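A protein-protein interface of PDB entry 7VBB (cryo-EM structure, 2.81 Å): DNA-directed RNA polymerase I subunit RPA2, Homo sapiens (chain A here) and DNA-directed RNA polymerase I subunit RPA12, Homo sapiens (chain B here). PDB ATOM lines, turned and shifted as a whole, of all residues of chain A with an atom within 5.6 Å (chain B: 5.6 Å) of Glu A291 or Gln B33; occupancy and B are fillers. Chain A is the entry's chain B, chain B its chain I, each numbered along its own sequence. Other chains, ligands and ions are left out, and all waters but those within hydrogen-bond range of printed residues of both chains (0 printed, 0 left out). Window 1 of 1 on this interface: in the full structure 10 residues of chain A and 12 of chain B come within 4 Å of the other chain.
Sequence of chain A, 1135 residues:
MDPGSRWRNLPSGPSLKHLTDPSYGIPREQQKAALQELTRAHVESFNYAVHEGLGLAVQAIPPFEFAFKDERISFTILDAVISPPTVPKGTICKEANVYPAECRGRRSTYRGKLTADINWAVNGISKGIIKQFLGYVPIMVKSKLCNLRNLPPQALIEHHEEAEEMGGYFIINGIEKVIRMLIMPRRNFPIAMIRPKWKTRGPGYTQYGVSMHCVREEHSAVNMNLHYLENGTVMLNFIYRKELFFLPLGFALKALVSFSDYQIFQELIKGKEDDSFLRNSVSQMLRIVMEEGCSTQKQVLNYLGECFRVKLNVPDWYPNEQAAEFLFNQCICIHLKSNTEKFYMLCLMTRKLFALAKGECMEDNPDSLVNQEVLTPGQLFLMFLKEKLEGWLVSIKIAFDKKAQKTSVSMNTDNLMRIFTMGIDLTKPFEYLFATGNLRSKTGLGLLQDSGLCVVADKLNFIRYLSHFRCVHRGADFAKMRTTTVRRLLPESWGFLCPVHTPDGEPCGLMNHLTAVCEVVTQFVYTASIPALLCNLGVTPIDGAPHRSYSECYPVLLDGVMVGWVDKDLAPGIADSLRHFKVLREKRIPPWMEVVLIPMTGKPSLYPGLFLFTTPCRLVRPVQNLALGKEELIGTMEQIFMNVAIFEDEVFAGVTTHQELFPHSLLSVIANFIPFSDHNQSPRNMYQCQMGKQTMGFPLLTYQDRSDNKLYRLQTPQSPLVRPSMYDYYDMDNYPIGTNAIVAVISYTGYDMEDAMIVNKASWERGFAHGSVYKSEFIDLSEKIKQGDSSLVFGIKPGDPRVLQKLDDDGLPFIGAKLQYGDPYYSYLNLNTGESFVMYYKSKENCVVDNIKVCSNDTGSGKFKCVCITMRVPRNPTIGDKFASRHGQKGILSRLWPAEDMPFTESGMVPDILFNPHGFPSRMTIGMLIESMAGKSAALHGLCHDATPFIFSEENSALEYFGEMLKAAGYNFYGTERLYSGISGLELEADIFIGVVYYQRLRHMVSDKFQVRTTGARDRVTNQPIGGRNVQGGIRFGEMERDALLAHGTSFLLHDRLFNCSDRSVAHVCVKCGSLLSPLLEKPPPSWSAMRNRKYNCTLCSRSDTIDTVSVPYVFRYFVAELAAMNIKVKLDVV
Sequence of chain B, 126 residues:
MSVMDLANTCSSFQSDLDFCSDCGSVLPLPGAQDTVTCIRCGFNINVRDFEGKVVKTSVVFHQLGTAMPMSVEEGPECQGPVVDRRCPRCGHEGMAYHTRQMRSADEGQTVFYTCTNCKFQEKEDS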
ATOM      1  N   LYS A 254     -25.026  12.827   6.106  1.00  0.00           N
ATOM      2  CA  LYS A 254     -25.083  14.269   6.465  1.00  0.00           C
ATOM      3  C   LYS A 254     -26.437  14.632   7.053  1.00  0.00           C
ATOM      4  O   LYS A 254     -26.466  15.483   7.927  1.00  0.00           O
ATOM      5  CB  LYS A 254     -24.813  15.129   5.235  1.00  0.00           C
ATOM      6  CG  LYS A 254     -23.349  15.234   4.834  1.00  0.00           C
ATOM      7  CD  LYS A 254     -22.632  16.391   5.482  1.00  0.00           C
ATOM      8  CE  LYS A 254     -22.701  17.649   4.648  1.00  0.00           C
ATOM      9  NZ  LYS A 254     -21.996  17.482   3.355  1.00  0.00           N
ATOM     10  N   LEU A 286     -18.523  12.264   0.259  1.00  0.00           N
ATOM     11  CA  LEU A 286     -18.866  13.507   0.989  1.00  0.00           C
ATOM     12  C   LEU A 286     -18.854  14.742   0.081  1.00  0.00           C
ATOM     13  O   LEU A 286     -19.708  15.603   0.259  1.00  0.00           O
ATOM     14  CB  LEU A 286     -17.922  13.646   2.184  1.00  0.00           C
ATOM     15  CG  LEU A 286     -17.932  12.460   3.131  1.00  0.00           C
ATOM     16  CD1 LEU A 286     -16.863  12.612   4.189  1.00  0.00           C
ATOM     17  CD2 LEU A 286     -19.304  12.308   3.755  1.00  0.00           C
ATOM     18  N   ARG A 287     -17.907  14.856  -0.832  1.00  0.00           N
ATOM     19  CA  ARG A 287     -17.787  16.100  -1.616  1.00  0.00           C
ATOM     20  C   ARG A 287     -18.507  16.001  -2.934  1.00  0.00           C
ATOM     21  O   ARG A 287     -19.270  16.902  -3.256  1.00  0.00           O
ATOM     22  CB  ARG A 287     -16.344  16.252  -2.087  1.00  0.00           C
ATOM     23  CG  ARG A 287     -16.135  17.225  -3.238  1.00  0.00           C
ATOM     24  CD  ARG A 287     -14.698  17.263  -3.712  1.00  0.00           C
ATOM     25  NE  ARG A 287     -14.091  15.953  -3.879  1.00  0.00           N
ATOM     26  CZ  ARG A 287     -13.023  15.534  -3.216  1.00  0.00           C
ATOM     27  NH1 ARG A 287     -12.438  16.325  -2.336  1.00  0.00           N
ATOM     28  NH2 ARG A 287     -12.539  14.329  -3.436  1.00  0.00           N
ATOM     29  N   ILE A 288     -18.339  14.904  -3.632  1.00  0.00           N
ATOM     30  CA  ILE A 288     -18.862  14.887  -5.023  1.00  0.00           C
ATOM     31  C   ILE A 288     -20.360  15.104  -5.044  1.00  0.00           C
ATOM     32  O   ILE A 288     -20.843  15.801  -5.944  1.00  0.00           O
ATOM     33  CB  ILE A 288     -18.358  13.716  -5.899  1.00  0.00           C
ATOM     34  CG1 ILE A 288     -16.902  13.931  -6.320  1.00  0.00           C
ATOM     35  CG2 ILE A 288     -19.250  13.471  -7.107  1.00  0.00           C
ATOM     36  CD1 ILE A 288     -16.679  15.144  -7.186  1.00  0.00           C
ATOM     37  N   VAL A 289     -21.085  14.552  -4.105  1.00  0.00           N
ATOM     38  CA  VAL A 289     -22.531  14.810  -4.304  1.00  0.00           C
ATOM     39  C   VAL A 289     -23.120  15.724  -3.227  1.00  0.00           C
ATOM     40  O   VAL A 289     -24.310  16.022  -3.332  1.00  0.00           O
ATOM     41  CB  VAL A 289     -23.300  13.500  -4.541  1.00  0.00           C
ATOM     42  CG1 VAL A 289     -24.253  13.620  -5.719  1.00  0.00           C
ATOM     43  CG2 VAL A 289     -22.355  12.331  -4.764  1.00  0.00           C
ATOM     44  N   MET A 290     -22.332  16.186  -2.266  1.00  0.00           N
ATOM     45  CA  MET A 290     -22.948  16.949  -1.155  1.00  0.00           C
ATOM     46  C   MET A 290     -22.389  18.361  -1.075  1.00  0.00           C
ATOM     47  O   MET A 290     -23.134  19.245  -0.708  1.00  0.00           O
ATOM     48  CB  MET A 290     -22.735  16.204   0.161  1.00  0.00           C
ATOM     49  CG  MET A 290     -23.681  15.062   0.347  1.00  0.00           C
ATOM     50  SD  MET A 290     -25.050  15.609   1.377  1.00  0.00           S
ATOM     51  CE  MET A 290     -25.917  16.718   0.276  1.00  0.00           C
ATOM     52  N   GLU A 291     -21.126  18.564  -1.422  1.00  0.00           N
ATOM     53  CA  GLU A 291     -20.578  19.937  -1.487  1.00  0.00           C
ATOM     54  C   GLU A 291     -21.145  20.499  -2.783  1.00  0.00           C
ATOM     55  O   GLU A 291     -20.898  21.667  -3.081  1.00  0.00           O
ATOM     56  CB  GLU A 291     -19.059  19.942  -1.417  1.00  0.00           C
ATOM     57  CG  GLU A 291     -18.493  21.221  -0.845  1.00  0.00           C
ATOM     58  CD  GLU A 291     -16.987  21.308  -0.979  1.00  0.00           C
ATOM     59  OE1 GLU A 291     -16.413  22.282  -0.469  1.00  0.00           O
ATOM     60  OE2 GLU A 291     -16.398  20.399  -1.594  1.00  0.00           O
ATOM     61  N   GLU A 292     -21.818  19.657  -3.559  1.00  0.00           N
ATOM     62  CA  GLU A 292     -22.558  20.177  -4.730  1.00  0.00           C
ATOM     63  C   GLU A 292     -23.934  20.675  -4.262  1.00  0.00           C
ATOM     64  O   GLU A 292     -24.921  19.969  -4.530  1.00  0.00           O
ATOM     65  CB  GLU A 292     -22.647  19.127  -5.833  1.00  0.00           C
ATOM     66  CG  GLU A 292     -21.505  19.196  -6.837  1.00  0.00           C
ATOM     67  CD  GLU A 292     -20.098  18.854  -6.368  1.00  0.00           C
ATOM     68  OE1 GLU A 292     -19.405  18.115  -7.093  1.00  0.00           O
ATOM     69  OE2 GLU A 292     -19.679  19.346  -5.305  1.00  0.00           O
ATOM     70  N   GLY A 293     -23.989  21.807  -3.538  1.00  0.00           N
ATOM     71  CA  GLY A 293     -25.254  22.479  -3.168  1.00  0.00           C
ATOM     72  C   GLY A 293     -25.691  22.463  -1.717  1.00  0.00           C
ATOM     73  O   GLY A 293     -26.271  23.474  -1.313  1.00  0.00           O
ATOM     74  N   CYS A 294     -25.392  21.423  -0.931  1.00  0.00           N
ATOM     75  CA  CYS A 294     -25.936  21.331   0.456  1.00  0.00           C
ATOM     76  C   CYS A 294     -24.843  21.056   1.481  1.00  0.00           C
ATOM     77  O   CYS A 294     -24.385  19.925   1.504  1.00  0.00           O
ATOM     78  CB  CYS A 294     -26.837  20.111   0.541  1.00  0.00           C
ATOM     79  SG  CYS A 294     -27.831  19.775  -0.932  1.00  0.00           S
ATOM     80  N   SER A 295     -24.521  21.975   2.382  1.00  0.00           N
ATOM     81  CA  SER A 295     -23.406  21.643   3.317  1.00  0.00           C
ATOM     82  C   SER A 295     -23.820  21.733   4.783  1.00  0.00           C
ATOM     83  O   SER A 295     -22.979  21.470   5.643  1.00  0.00           O
ATOM     84  CB  SER A 295     -22.176  22.446   3.055  1.00  0.00           C
ATOM     85  OG  SER A 295     -21.016  21.734   3.458  1.00  0.00           O
ATOM     86  N   GLN A 299     -29.891  21.904   4.818  1.00  0.00           N
ATOM     87  CA  GLN A 299     -29.983  22.010   3.342  1.00  0.00           C
ATOM     88  C   GLN A 299     -30.047  20.605   2.771  1.00  0.00           C
ATOM     89  O   GLN A 299     -30.748  20.408   1.773  1.00  0.00           O
ATOM     90  CB  GLN A 299     -28.910  22.875   2.691  1.00  0.00           C
ATOM     91  CG  GLN A 299     -28.961  24.345   3.056  1.00  0.00           C
ATOM     92  CD  GLN A 299     -27.706  25.025   2.569  1.00  0.00           C
ATOM     93  OE1 GLN A 299     -27.232  24.767   1.467  1.00  0.00           O
ATOM     94  NE2 GLN A 299     -27.149  25.895   3.396  1.00  0.00           N
ATOM     95  N   GLN B  14     -11.337  20.803   6.070  1.00  0.00           N
ATOM     96  CA  GLN B  14     -11.062  22.213   6.342  1.00  0.00           C
ATOM     97  C   GLN B  14     -10.114  22.399   7.525  1.00  0.00           C
ATOM     98  O   GLN B  14      -9.334  23.356   7.554  1.00  0.00           O
ATOM     99  CB  GLN B  14     -12.377  22.959   6.565  1.00  0.00           C
ATOM    100  CG  GLN B  14     -12.898  23.647   5.309  1.00  0.00           C
ATOM    101  CD  GLN B  14     -14.403  23.833   5.304  1.00  0.00           C
ATOM    102  OE1 GLN B  14     -15.140  23.058   5.910  1.00  0.00           O
ATOM    103  NE2 GLN B  14     -14.868  24.863   4.613  1.00  0.00           N
ATOM    104  N   CYS B  20     -15.223  18.690   3.868  1.00  0.00           N
ATOM    105  CA  CYS B  20     -14.067  18.343   3.058  1.00  0.00           C
ATOM    106  C   CYS B  20     -13.894  19.337   1.919  1.00  0.00           C
ATOM    107  O   CYS B  20     -14.865  19.782   1.302  1.00  0.00           O
ATOM    108  CB  CYS B  20     -14.209  16.930   2.493  1.00  0.00           C
ATOM    109  SG  CYS B  20     -15.586  16.722   1.356  1.00  0.00           S
ATOM    110  N   SER B  21     -12.608  20.342   1.482  1.00  0.00           N
ATOM    111  CA  SER B  21     -12.266  21.258   0.404  1.00  0.00           C
ATOM    112  C   SER B  21     -12.582  20.598  -0.936  1.00  0.00           C
ATOM    113  O   SER B  21     -13.158  19.508  -1.000  1.00  0.00           O
ATOM    114  CB  SER B  21     -10.801  21.666   0.507  1.00  0.00           C
ATOM    115  OG  SER B  21     -10.553  22.372   1.708  1.00  0.00           O
ATOM    116  N   ASP B  22     -12.353  21.352  -2.013  1.00  0.00           N
ATOM    117  CA  ASP B  22     -12.628  20.822  -3.372  1.00  0.00           C
ATOM    118  C   ASP B  22     -11.302  20.465  -4.051  1.00  0.00           C
ATOM    119  O   ASP B  22     -10.258  20.672  -3.429  1.00  0.00           O
ATOM    120  CB  ASP B  22     -13.471  21.816  -4.165  1.00  0.00           C
ATOM    121  CG  ASP B  22     -14.419  21.163  -5.154  1.00  0.00           C
ATOM    122  OD1 ASP B  22     -14.036  20.135  -5.746  1.00  0.00           O
ATOM    123  OD2 ASP B  22     -15.542  21.683  -5.319  1.00  0.00           O
ATOM    124  N   GLY B  31     -10.744  27.458  -1.134  1.00  0.00           N
ATOM    125  CA  GLY B  31     -11.743  27.768  -0.102  1.00  0.00           C
ATOM    126  C   GLY B  31     -13.046  27.035  -0.343  1.00  0.00           C
ATOM    127  O   GLY B  31     -13.575  27.135  -1.470  1.00  0.00           O
ATOM    128  N   ALA B  32     -13.578  26.371   0.676  1.00  0.00           N
ATOM    129  CA  ALA B  32     -14.806  25.606   0.572  1.00  0.00           C
ATOM    130  C   ALA B  32     -16.004  26.538   0.427  1.00  0.00           C
ATOM    131  O   ALA B  32     -15.946  27.727   0.752  1.00  0.00           O
ATOM    132  CB  ALA B  32     -14.986  24.700   1.790  1.00  0.00           C
ATOM    133  N   GLN B  33     -17.104  25.973  -0.074  1.00  0.00           N
ATOM    134  CA  GLN B  33     -18.321  26.754  -0.274  1.00  0.00           C
ATOM    135  C   GLN B  33     -18.758  27.451   1.008  1.00  0.00           C
ATOM    136  O   GLN B  33     -19.515  28.428   0.964  1.00  0.00           O
ATOM    137  CB  GLN B  33     -19.429  25.848  -0.805  1.00  0.00           C
ATOM    138  CG  GLN B  33     -20.112  25.008   0.257  1.00  0.00           C
ATOM    139  CD  GLN B  33     -21.478  24.514  -0.178  1.00  0.00           C
ATOM    140  OE1 GLN B  33     -21.634  23.968  -1.270  1.00  0.00           O
ATOM    141  NE2 GLN B  33     -22.474  24.701   0.679  1.00  0.00           N
ATOM    142  N   ASP B  34     -18.304  26.965   2.158  1.00  0.00           N
ATOM    143  CA  ASP B  34     -18.626  27.555   3.452  1.00  0.00           C
ATOM    144  C   ASP B  34     -17.326  27.941   4.142  1.00  0.00           C
ATOM    145  O   ASP B  34     -16.409  27.119   4.240  1.00  0.00           O
ATOM    146  CB  ASP B  34     -19.411  26.568   4.315  1.00  0.00           C
ATOM    147  CG  ASP B  34     -20.661  26.059   3.630  1.00  0.00           C
ATOM    148  OD1 ASP B  34     -20.991  26.560   2.535  1.00  0.00           O
ATOM    149  OD2 ASP B  34     -21.320  25.164   4.197  1.00  0.00           O
ATOM    150  N   THR B  35     -17.254  29.178   4.641  1.00  0.00           N
ATOM    151  CA  THR B  35     -16.069  29.596   5.382  1.00  0.00           C
ATOM    152  C   THR B  35     -14.821  29.490   4.511  1.00  0.00           C
ATOM    153  O   THR B  35     -14.031  28.555   4.660  1.00  0.00           O
ATOM    154  CB  THR B  35     -15.908  28.764   6.654  1.00  0.00           C
ATOM    155  OG1 THR B  35     -15.777  27.380   6.310  1.00  0.00           O
ATOM    156  CG2 THR B  35     -17.114  28.935   7.557  1.00  0.00           C
ATOM    157  N   VAL B  36     -14.640  30.432   3.591  1.00  0.00           N
ATOM    158  CA  VAL B  36     -13.706  30.267   2.483  1.00  0.00           C
ATOM    159  C   VAL B  36     -12.253  30.507   2.874  1.00  0.00           C
ATOM    160  O   VAL B  36     -11.395  30.562   1.982  1.00  0.00           O
ATOM    161  CB  VAL B  36     -14.093  31.178   1.296  1.00  0.00           C
ATOM    162  CG1 VAL B  36     -13.278  30.844   0.054  1.00  0.00           C
ATOM    163  CG2 VAL B  36     -15.579  31.066   1.016  1.00  0.00           C
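Hydrophobic or aromatic side chains of chain B within 4 Å of the printed part of chain A: Ala B32.
Of the 12 printed residues of chain A, 5 touch a printed residue of chain B.
Among the printed residues, no Asp or Glu carboxylate lies within 4 Å of a Lys or Arg side-chain nitrogen of the other chain.
The backbone carbonyl oxygen (O) of Glu A291 lies close to the side-chain amide oxygen (OE1) of Gln B33 (3.0 Å).
The side-chain carboxylate (OE2) of Glu A291 lies close to the backbone carbonyl oxygen (O) of Ser B21, 3.4 Å away.
SG of Cys B20 sits close to N of Arg A287 (3.7 Å).
The backbone carbonyl oxygen (O) of Cys B20 sits close to the side-chain carboxylate (OE2) of Glu A291 (3.3 Å).
NE2 of Gln B14 is in hydrogen-bond range of O of Asp B34 (2.8 Å).
The backbone carbonyl oxygen of Gly A293 lies close to the side-chain amide oxygen of Gln A299.
The side-chain amide nitrogen (NE2) of Gln B33 lies close to the side-chain carboxylate (OD1) of Asp B34 (3.0 Å).
Leu A286 touches Cys B20 (CB to SG, 3.95 Å).
Ser B21 touches Arg A287.
Arg A287 touches Asp B22 (CD to OD1, 3.6 Å).
Glu A291 touches Ala B32.
Gly A293 touches Gln B33.
Gln B33 touches Ser A295 (NE2 to CB, 3.3 Å).
Ser A295 touches Asp B34.
Glu A291 touches four residues of chain B.
Printed residues of chain A within 4 Å of Ser B21: Arg A287 and Glu A291.
Printed residues of chain B within 4 Å of Ser A295: Gln B33 (3.3 Å) and Asp B34 (3.1 Å).
Printed residues of chain B within 4 Å of Arg A287: Cys B20, Ser B21 and Asp B22.
Printed residues of chain A within 4 Å of Asp B34: Ser A295 (3.1 Å).
The nearest residue of chain A that does not touch Gln B33 is Cys A294 (4.4 Å).
The nearest printed residue of chain B that does not touch Leu A286 is Ser B21 (7.5 Å).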
